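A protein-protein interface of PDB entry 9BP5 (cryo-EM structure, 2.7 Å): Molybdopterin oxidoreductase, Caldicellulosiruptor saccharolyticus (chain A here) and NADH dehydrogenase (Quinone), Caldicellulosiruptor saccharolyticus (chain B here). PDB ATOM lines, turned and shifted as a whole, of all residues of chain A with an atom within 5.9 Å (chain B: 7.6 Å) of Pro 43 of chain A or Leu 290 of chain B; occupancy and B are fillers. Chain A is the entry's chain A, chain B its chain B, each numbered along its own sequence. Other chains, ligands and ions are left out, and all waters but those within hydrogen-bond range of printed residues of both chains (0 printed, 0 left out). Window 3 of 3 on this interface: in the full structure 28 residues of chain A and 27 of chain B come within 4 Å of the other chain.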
ATOM      1  N   LEU A  41      -1.969   8.096  20.262  1.00  0.00           N
ATOM      2  CA  LEU A  41      -1.404   8.107  18.927  1.00  0.00           C
ATOM      3  C   LEU A  41      -1.932   6.932  18.118  1.00  0.00           C
ATOM      4  O   LEU A  41      -2.365   5.915  18.664  1.00  0.00           O
ATOM      5  CB  LEU A  41       0.128   8.061  18.979  1.00  0.00           C
ATOM      6  CG  LEU A  41       0.809   8.946  20.023  1.00  0.00           C
ATOM      7  CD1 LEU A  41       2.284   8.644  20.082  1.00  0.00           C
ATOM      8  CD2 LEU A  41       0.577  10.410  19.726  1.00  0.00           C
ATOM      9  N   LYS A  42      -1.906   7.096  16.800  1.00  0.00           N
ATOM     10  CA  LYS A  42      -2.233   6.002  15.907  1.00  0.00           C
ATOM     11  C   LYS A  42      -1.163   4.917  16.006  1.00  0.00           C
ATOM     12  O   LYS A  42      -0.005   5.206  16.317  1.00  0.00           O
ATOM     13  CB  LYS A  42      -2.342   6.501  14.472  1.00  0.00           C
ATOM     14  CG  LYS A  42      -3.306   7.654  14.289  1.00  0.00           C
ATOM     15  CD  LYS A  42      -2.977   8.454  13.042  1.00  0.00           C
ATOM     16  CE  LYS A  42      -1.563   9.001  13.096  1.00  0.00           C
ATOM     17  NZ  LYS A  42      -1.093   9.481  11.771  1.00  0.00           N
ATOM     18  N   PRO A  43      -1.523   3.659  15.754  1.00  0.00           N
ATOM     19  CA  PRO A  43      -0.539   2.578  15.876  1.00  0.00           C
ATOM     20  C   PRO A  43       0.601   2.738  14.884  1.00  0.00           C
ATOM     21  O   PRO A  43       0.451   3.339  13.818  1.00  0.00           O
ATOM     22  CB  PRO A  43      -1.360   1.316  15.595  1.00  0.00           C
ATOM     23  CG  PRO A  43      -2.766   1.710  15.875  1.00  0.00           C
ATOM     24  CD  PRO A  43      -2.869   3.144  15.461  1.00  0.00           C
ATOM     25  N   TYR A  44       1.757   2.210  15.265  1.00  0.00           N
ATOM     26  CA  TYR A  44       3.009   2.384  14.544  1.00  0.00           C
ATOM     27  C   TYR A  44       3.661   1.072  14.138  1.00  0.00           C
ATOM     28  O   TYR A  44       4.260   0.998  13.065  1.00  0.00           O
ATOM     29  CB  TYR A  44       3.977   3.191  15.405  1.00  0.00           C
ATOM     30  CG  TYR A  44       5.106   3.838  14.652  1.00  0.00           C
ATOM     31  CD1 TYR A  44       4.865   4.657  13.564  1.00  0.00           C
ATOM     32  CD2 TYR A  44       6.415   3.646  15.045  1.00  0.00           C
ATOM     33  CE1 TYR A  44       5.895   5.248  12.886  1.00  0.00           C
ATOM     34  CE2 TYR A  44       7.450   4.231  14.371  1.00  0.00           C
ATOM     35  CZ  TYR A  44       7.188   5.032  13.296  1.00  0.00           C
ATOM     36  OH  TYR A  44       8.234   5.615  12.627  1.00  0.00           O
ATOM     37  N   GLY A  45       3.570   0.037  14.969  1.00  0.00           N
ATOM     38  CA  GLY A  45       4.040  -1.279  14.588  1.00  0.00           C
ATOM     39  C   GLY A  45       5.538  -1.420  14.481  1.00  0.00           C
ATOM     40  O   GLY A  45       6.018  -2.328  13.801  1.00  0.00           O
ATOM     41  N   ARG A  62       0.398  -8.110  15.861  1.00  0.00           N
ATOM     42  CA  ARG A  62       0.689  -7.051  16.817  1.00  0.00           C
ATOM     43  C   ARG A  62      -0.557  -6.735  17.627  1.00  0.00           C
ATOM     44  O   ARG A  62      -1.589  -6.356  17.067  1.00  0.00           O
ATOM     45  CB  ARG A  62       1.186  -5.810  16.089  1.00  0.00           C
ATOM     46  CG  ARG A  62       2.580  -5.957  15.542  1.00  0.00           C
ATOM     47  CD  ARG A  62       2.784  -5.132  14.296  1.00  0.00           C
ATOM     48  NE  ARG A  62       4.199  -4.873  14.064  1.00  0.00           N
ATOM     49  CZ  ARG A  62       5.059  -5.760  13.580  1.00  0.00           C
ATOM     50  NH1 ARG A  62       4.677  -6.979  13.237  1.00  0.00           N
ATOM     51  NH2 ARG A  62       6.335  -5.413  13.436  1.00  0.00           N
ATOM     52  N   CYS A  64      -1.083  -4.270  19.520  1.00  0.00           N
ATOM     53  CA  CYS A  64      -1.376  -2.843  19.546  1.00  0.00           C
ATOM     54  C   CYS A  64      -2.227  -2.388  18.370  1.00  0.00           C
ATOM     55  O   CYS A  64      -2.861  -1.332  18.458  1.00  0.00           O
ATOM     56  CB  CYS A  64      -0.074  -2.040  19.570  1.00  0.00           C
ATOM     57  SG  CYS A  64       0.900  -2.102  18.050  1.00  0.00           S
ATOM     58  N   SER A  65      -2.258  -3.151  17.280  1.00  0.00           N
ATOM     59  CA  SER A  65      -2.994  -2.757  16.090  1.00  0.00           C
ATOM     60  C   SER A  65      -4.048  -3.760  15.652  1.00  0.00           C
ATOM     61  O   SER A  65      -4.886  -3.416  14.815  1.00  0.00           O
ATOM     62  CB  SER A  65      -2.028  -2.511  14.922  1.00  0.00           C
ATOM     63  OG  SER A  65      -1.156  -3.607  14.739  1.00  0.00           O
ATOM     64  N   TYR A  67      -7.448  -5.841  16.137  1.00  0.00           N
ATOM     65  CA  TYR A  67      -8.705  -5.674  16.845  1.00  0.00           C
ATOM     66  C   TYR A  67      -9.287  -7.028  17.217  1.00  0.00           C
ATOM     67  O   TYR A  67      -9.142  -8.009  16.485  1.00  0.00           O
ATOM     68  CB  TYR A  67      -9.705  -4.888  15.996  1.00  0.00           C
ATOM     69  CG  TYR A  67      -9.354  -3.429  15.876  1.00  0.00           C
ATOM     70  CD1 TYR A  67      -9.767  -2.519  16.831  1.00  0.00           C
ATOM     71  CD2 TYR A  67      -8.591  -2.965  14.816  1.00  0.00           C
ATOM     72  CE1 TYR A  67      -9.440  -1.188  16.733  1.00  0.00           C
ATOM     73  CE2 TYR A  67      -8.258  -1.637  14.709  1.00  0.00           C
ATOM     74  CZ  TYR A  67      -8.687  -0.751  15.670  1.00  0.00           C
ATOM     75  OH  TYR A  67      -8.361   0.580  15.567  1.00  0.00           O
ATOM     76  N   ARG A 621       6.054  11.344  17.183  1.00  0.00           N
ATOM     77  CA  ARG A 621       4.615  11.197  17.044  1.00  0.00           C
ATOM     78  C   ARG A 621       3.863  12.031  18.065  1.00  0.00           C
ATOM     79  O   ARG A 621       2.761  12.500  17.780  1.00  0.00           O
ATOM     80  CB  ARG A 621       4.235   9.725  17.162  1.00  0.00           C
ATOM     81  CG  ARG A 621       4.635   8.899  15.959  1.00  0.00           C
ATOM     82  CD  ARG A 621       5.037   7.503  16.354  1.00  0.00           C
ATOM     83  NE  ARG A 621       3.912   6.738  16.873  1.00  0.00           N
ATOM     84  CZ  ARG A 621       4.026   5.693  17.679  1.00  0.00           C
ATOM     85  NH1 ARG A 621       5.205   5.260  18.085  1.00  0.00           N
ATOM     86  NH2 ARG A 621       2.927   5.067  18.085  1.00  0.00           N
ATOM     87  N   GLU B 273       6.536  -0.532  -2.028  1.00  0.00           N
ATOM     88  CA  GLU B 273       5.443  -1.060  -1.229  1.00  0.00           C
ATOM     89  C   GLU B 273       4.223  -0.156  -1.350  1.00  0.00           C
ATOM     90  O   GLU B 273       4.341   1.059  -1.523  1.00  0.00           O
ATOM     91  CB  GLU B 273       5.864  -1.184   0.232  1.00  0.00           C
ATOM     92  CG  GLU B 273       5.277  -2.377   0.948  1.00  0.00           C
ATOM     93  CD  GLU B 273       4.055  -2.016   1.759  1.00  0.00           C
ATOM     94  OE1 GLU B 273       3.641  -0.839   1.712  1.00  0.00           O
ATOM     95  OE2 GLU B 273       3.512  -2.901   2.450  1.00  0.00           O
ATOM     96  N   THR B 275       1.754   0.769   0.822  1.00  0.00           N
ATOM     97  CA  THR B 275       1.596   1.766   1.871  1.00  0.00           C
ATOM     98  C   THR B 275       2.774   2.725   1.962  1.00  0.00           C
ATOM     99  O   THR B 275       2.665   3.745   2.648  1.00  0.00           O
ATOM    100  CB  THR B 275       1.385   1.078   3.212  1.00  0.00           C
ATOM    101  OG1 THR B 275       2.353   0.035   3.367  1.00  0.00           O
ATOM    102  CG2 THR B 275      -0.003   0.485   3.283  1.00  0.00           C
ATOM    103  N   MET B 287       7.565   5.627   4.750  1.00  0.00           N
ATOM    104  CA  MET B 287       7.576   4.623   5.801  1.00  0.00           C
ATOM    105  C   MET B 287       6.297   3.810   5.722  1.00  0.00           C
ATOM    106  O   MET B 287       5.207   4.386   5.857  1.00  0.00           O
ATOM    107  CB  MET B 287       7.699   5.279   7.170  1.00  0.00           C
ATOM    108  CG  MET B 287       9.124   5.491   7.638  1.00  0.00           C
ATOM    109  SD  MET B 287       9.214   5.848   9.400  1.00  0.00           S
ATOM    110  CE  MET B 287      10.968   5.646   9.702  1.00  0.00           C
ATOM    111  N   PRO B 288       6.369   2.501   5.497  1.00  0.00           N
ATOM    112  CA  PRO B 288       5.147   1.705   5.348  1.00  0.00           C
ATOM    113  C   PRO B 288       4.247   1.793   6.568  1.00  0.00           C
ATOM    114  O   PRO B 288       4.708   1.786   7.710  1.00  0.00           O
ATOM    115  CB  PRO B 288       5.684   0.287   5.150  1.00  0.00           C
ATOM    116  CG  PRO B 288       6.988   0.494   4.508  1.00  0.00           C
ATOM    117  CD  PRO B 288       7.565   1.726   5.141  1.00  0.00           C
ATOM    118  N   ARG B 289       2.946   1.869   6.313  1.00  0.00           N
ATOM    119  CA  ARG B 289       1.946   1.955   7.362  1.00  0.00           C
ATOM    120  C   ARG B 289       1.521   0.544   7.756  1.00  0.00           C
ATOM    121  O   ARG B 289       2.045  -0.449   7.249  1.00  0.00           O
ATOM    122  CB  ARG B 289       0.763   2.798   6.894  1.00  0.00           C
ATOM    123  CG  ARG B 289       0.974   4.297   7.019  1.00  0.00           C
ATOM    124  CD  ARG B 289       1.679   4.852   5.794  1.00  0.00           C
ATOM    125  NE  ARG B 289       1.540   6.296   5.678  1.00  0.00           N
ATOM    126  CZ  ARG B 289       0.491   6.906   5.145  1.00  0.00           C
ATOM    127  NH1 ARG B 289      -0.535   6.225   4.666  1.00  0.00           N
ATOM    128  NH2 ARG B 289       0.473   8.234   5.089  1.00  0.00           N
ATOM    129  N   LEU B 290       0.562   0.441   8.667  1.00  0.00           N
ATOM    130  CA  LEU B 290       0.039  -0.851   9.065  1.00  0.00           C
ATOM    131  C   LEU B 290      -1.025  -1.296   8.065  1.00  0.00           C
ATOM    132  O   LEU B 290      -1.453  -0.533   7.197  1.00  0.00           O
ATOM    133  CB  LEU B 290      -0.497  -0.784  10.493  1.00  0.00           C
ATOM    134  CG  LEU B 290       0.598  -0.963  11.548  1.00  0.00           C
ATOM    135  CD1 LEU B 290       0.137  -0.469  12.904  1.00  0.00           C
ATOM    136  CD2 LEU B 290       1.035  -2.419  11.626  1.00  0.00           C
ATOM    137  N   LYS B 291      -1.452  -2.548   8.176  1.00  0.00           N
ATOM    138  CA  LYS B 291      -2.296  -3.115   7.131  1.00  0.00           C
ATOM    139  C   LYS B 291      -3.704  -2.522   7.140  1.00  0.00           C
ATOM    140  O   LYS B 291      -4.213  -2.174   6.069  1.00  0.00           O
ATOM    141  CB  LYS B 291      -2.335  -4.643   7.237  1.00  0.00           C
ATOM    142  CG  LYS B 291      -1.038  -5.337   6.816  1.00  0.00           C
ATOM    143  CD  LYS B 291      -0.354  -4.651   5.631  1.00  0.00           C
ATOM    144  CE  LYS B 291      -1.169  -4.755   4.344  1.00  0.00           C
ATOM    145  NZ  LYS B 291      -0.653  -3.842   3.288  1.00  0.00           N
ATOM    146  N   PRO B 292      -4.375  -2.391   8.284  1.00  0.00           N
ATOM    147  CA  PRO B 292      -5.637  -1.648   8.300  1.00  0.00           C
ATOM    148  C   PRO B 292      -5.381  -0.164   8.475  1.00  0.00           C
ATOM    149  O   PRO B 292      -4.646   0.242   9.388  1.00  0.00           O
ATOM    150  CB  PRO B 292      -6.380  -2.231   9.514  1.00  0.00           C
ATOM    151  CG  PRO B 292      -5.623  -3.469   9.884  1.00  0.00           C
ATOM    152  CD  PRO B 292      -4.211  -3.143   9.537  1.00  0.00           C
ATOM    153  N   PRO B 293      -5.966   0.683   7.625  1.00  0.00           N
ATOM    154  CA  PRO B 293      -6.841   0.368   6.495  1.00  0.00           C
ATOM    155  C   PRO B 293      -6.059   0.016   5.235  1.00  0.00           C
ATOM    156  O   PRO B 293      -4.921   0.440   5.058  1.00  0.00           O
ATOM    157  CB  PRO B 293      -7.646   1.656   6.335  1.00  0.00           C
ATOM    158  CG  PRO B 293      -6.674   2.742   6.718  1.00  0.00           C
ATOM    159  CD  PRO B 293      -5.707   2.130   7.714  1.00  0.00           C
ATOM    160  N   PHE B 294      -6.657  -0.768   4.343  1.00  0.00           N
ATOM    161  CA  PHE B 294      -5.969  -1.234   3.148  1.00  0.00           C
ATOM    162  C   PHE B 294      -6.038  -0.176   2.049  1.00  0.00           C
ATOM    163  O   PHE B 294      -6.953   0.649   2.040  1.00  0.00           O
ATOM    164  CB  PHE B 294      -6.582  -2.540   2.652  1.00  0.00           C
ATOM    165  CG  PHE B 294      -6.385  -3.694   3.589  1.00  0.00           C
ATOM    166  CD1 PHE B 294      -7.037  -3.735   4.810  1.00  0.00           C
ATOM    167  CD2 PHE B 294      -5.534  -4.732   3.256  1.00  0.00           C
ATOM    168  CE1 PHE B 294      -6.851  -4.791   5.675  1.00  0.00           C
ATOM    169  CE2 PHE B 294      -5.345  -5.791   4.117  1.00  0.00           C
ATOM    170  CZ  PHE B 294      -6.003  -5.821   5.328  1.00  0.00           C
ATOM    171  N   PRO B 295      -5.078  -0.172   1.122  1.00  0.00           N
ATOM    172  CA  PRO B 295      -5.117   0.817   0.032  1.00  0.00           C
ATOM    173  C   PRO B 295      -6.389   0.771  -0.795  1.00  0.00           C
ATOM    174  O   PRO B 295      -6.856   1.818  -1.257  1.00  0.00           O
ATOM    175  CB  PRO B 295      -3.885   0.449  -0.801  1.00  0.00           C
ATOM    176  CG  PRO B 295      -2.945  -0.136   0.179  1.00  0.00           C
ATOM    177  CD  PRO B 295      -3.796  -0.895   1.159  1.00  0.00           C
ATOM    178  N   LYS B 444      12.269   1.301  10.328  1.00  0.00           N
ATOM    179  CA  LYS B 444      11.216   1.569  11.300  1.00  0.00           C
ATOM    180  C   LYS B 444      11.096   0.466  12.343  1.00  0.00           C
ATOM    181  O   LYS B 444      11.010   0.755  13.539  1.00  0.00           O
ATOM    182  CB  LYS B 444       9.871   1.762  10.591  1.00  0.00           C
ATOM    183  CG  LYS B 444       8.667   1.643  11.508  1.00  0.00           C
ATOM    184  CD  LYS B 444       7.362   1.652  10.730  1.00  0.00           C
ATOM    185  CE  LYS B 444       7.162   2.970  10.009  1.00  0.00           C
ATOM    186  NZ  LYS B 444       5.723   3.340   9.904  1.00  0.00           N
ATOM    187  N   LEU B 487       7.564  -5.798   9.635  1.00  0.00           N
ATOM    188  CA  LEU B 487       6.294  -5.136   9.356  1.00  0.00           C
ATOM    189  C   LEU B 487       5.884  -5.301   7.898  1.00  0.00           C
ATOM    190  O   LEU B 487       4.836  -5.881   7.597  1.00  0.00           O
ATOM    191  CB  LEU B 487       6.394  -3.652   9.715  1.00  0.00           C
ATOM    192  CG  LEU B 487       5.159  -2.934  10.258  1.00  0.00           C
ATOM    193  CD1 LEU B 487       5.534  -1.532  10.696  1.00  0.00           C
ATOM    194  CD2 LEU B 487       4.041  -2.883   9.233  1.00  0.00           C
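The side-chain hydroxyl (OH) of Tyr 44 of chain A lies within hydrogen-bond range of the side-chain sulfur (SD) of Met 287 of chain B, at 3.4 Å.
The guanidinium group (NH2) of Arg 62 of chain A sits at hydrogen-bond distance from the backbone carbonyl oxygen (O) of Gly 45 of chain A, 3.1 Å away. The backbone carbonyl oxygen of Pro 288 of chain B is in hydrogen-bond range of the side-chain amino group of Lys 444 of chain B, 2.9 Å away.
CB of Pro 43 of chain A touches CD1 of Leu 290 of chain B, 3.6 Å away. Leu 290 of chain B touches Tyr 44 of chain A (CD1 to N, 3.9 Å). Lys 444 of chain B touches Tyr 44 of chain A (NZ to CE1, 3.5 Å). Tyr 44 of chain A touches Leu 487 of chain B. O of Gly 45 of chain A touches CD1 of Leu 487 of chain B (3.2 Å). CB of Ser 65 of chain A touches CD1 of Leu 290 of chain B, at 3.6 Å.
Of the printed residues of chain B, Pro 43 of chain A touches Leu 290. Of the printed residues of chain A, Leu 290 of chain B touches Pro 43 (3.6 Å), Tyr 44 (3.9 Å) and Ser 65 (3.6 Å). Of the printed residues of chain A, Leu 487 of chain B touches Tyr 44 (3.7 Å) and Gly 45 (3.2 Å). Printed residues of chain B within 4 Å of Tyr 44 of chain A: Met 287 (3.4 Å), Leu 290 (3.9 Å), Lys 444 (3.5 Å) and Leu 487 (3.7 Å). The nearest printed residue of chain A that does not touch Met 287 of chain B is Arg 621 of chain A (8.3 Å).
Of the 10 printed residues of chain A, 4 touch a printed residue of chain B. Along chain A the printed residues that touch a printed residue of chain B span positions 43 to 65. Among the printed residues, 7 pairs touch across the chains. Among the printed residues, no Asp or Glu carboxylate lies within 4 Å of a Lys or Arg side-chain nitrogen of the other chain.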
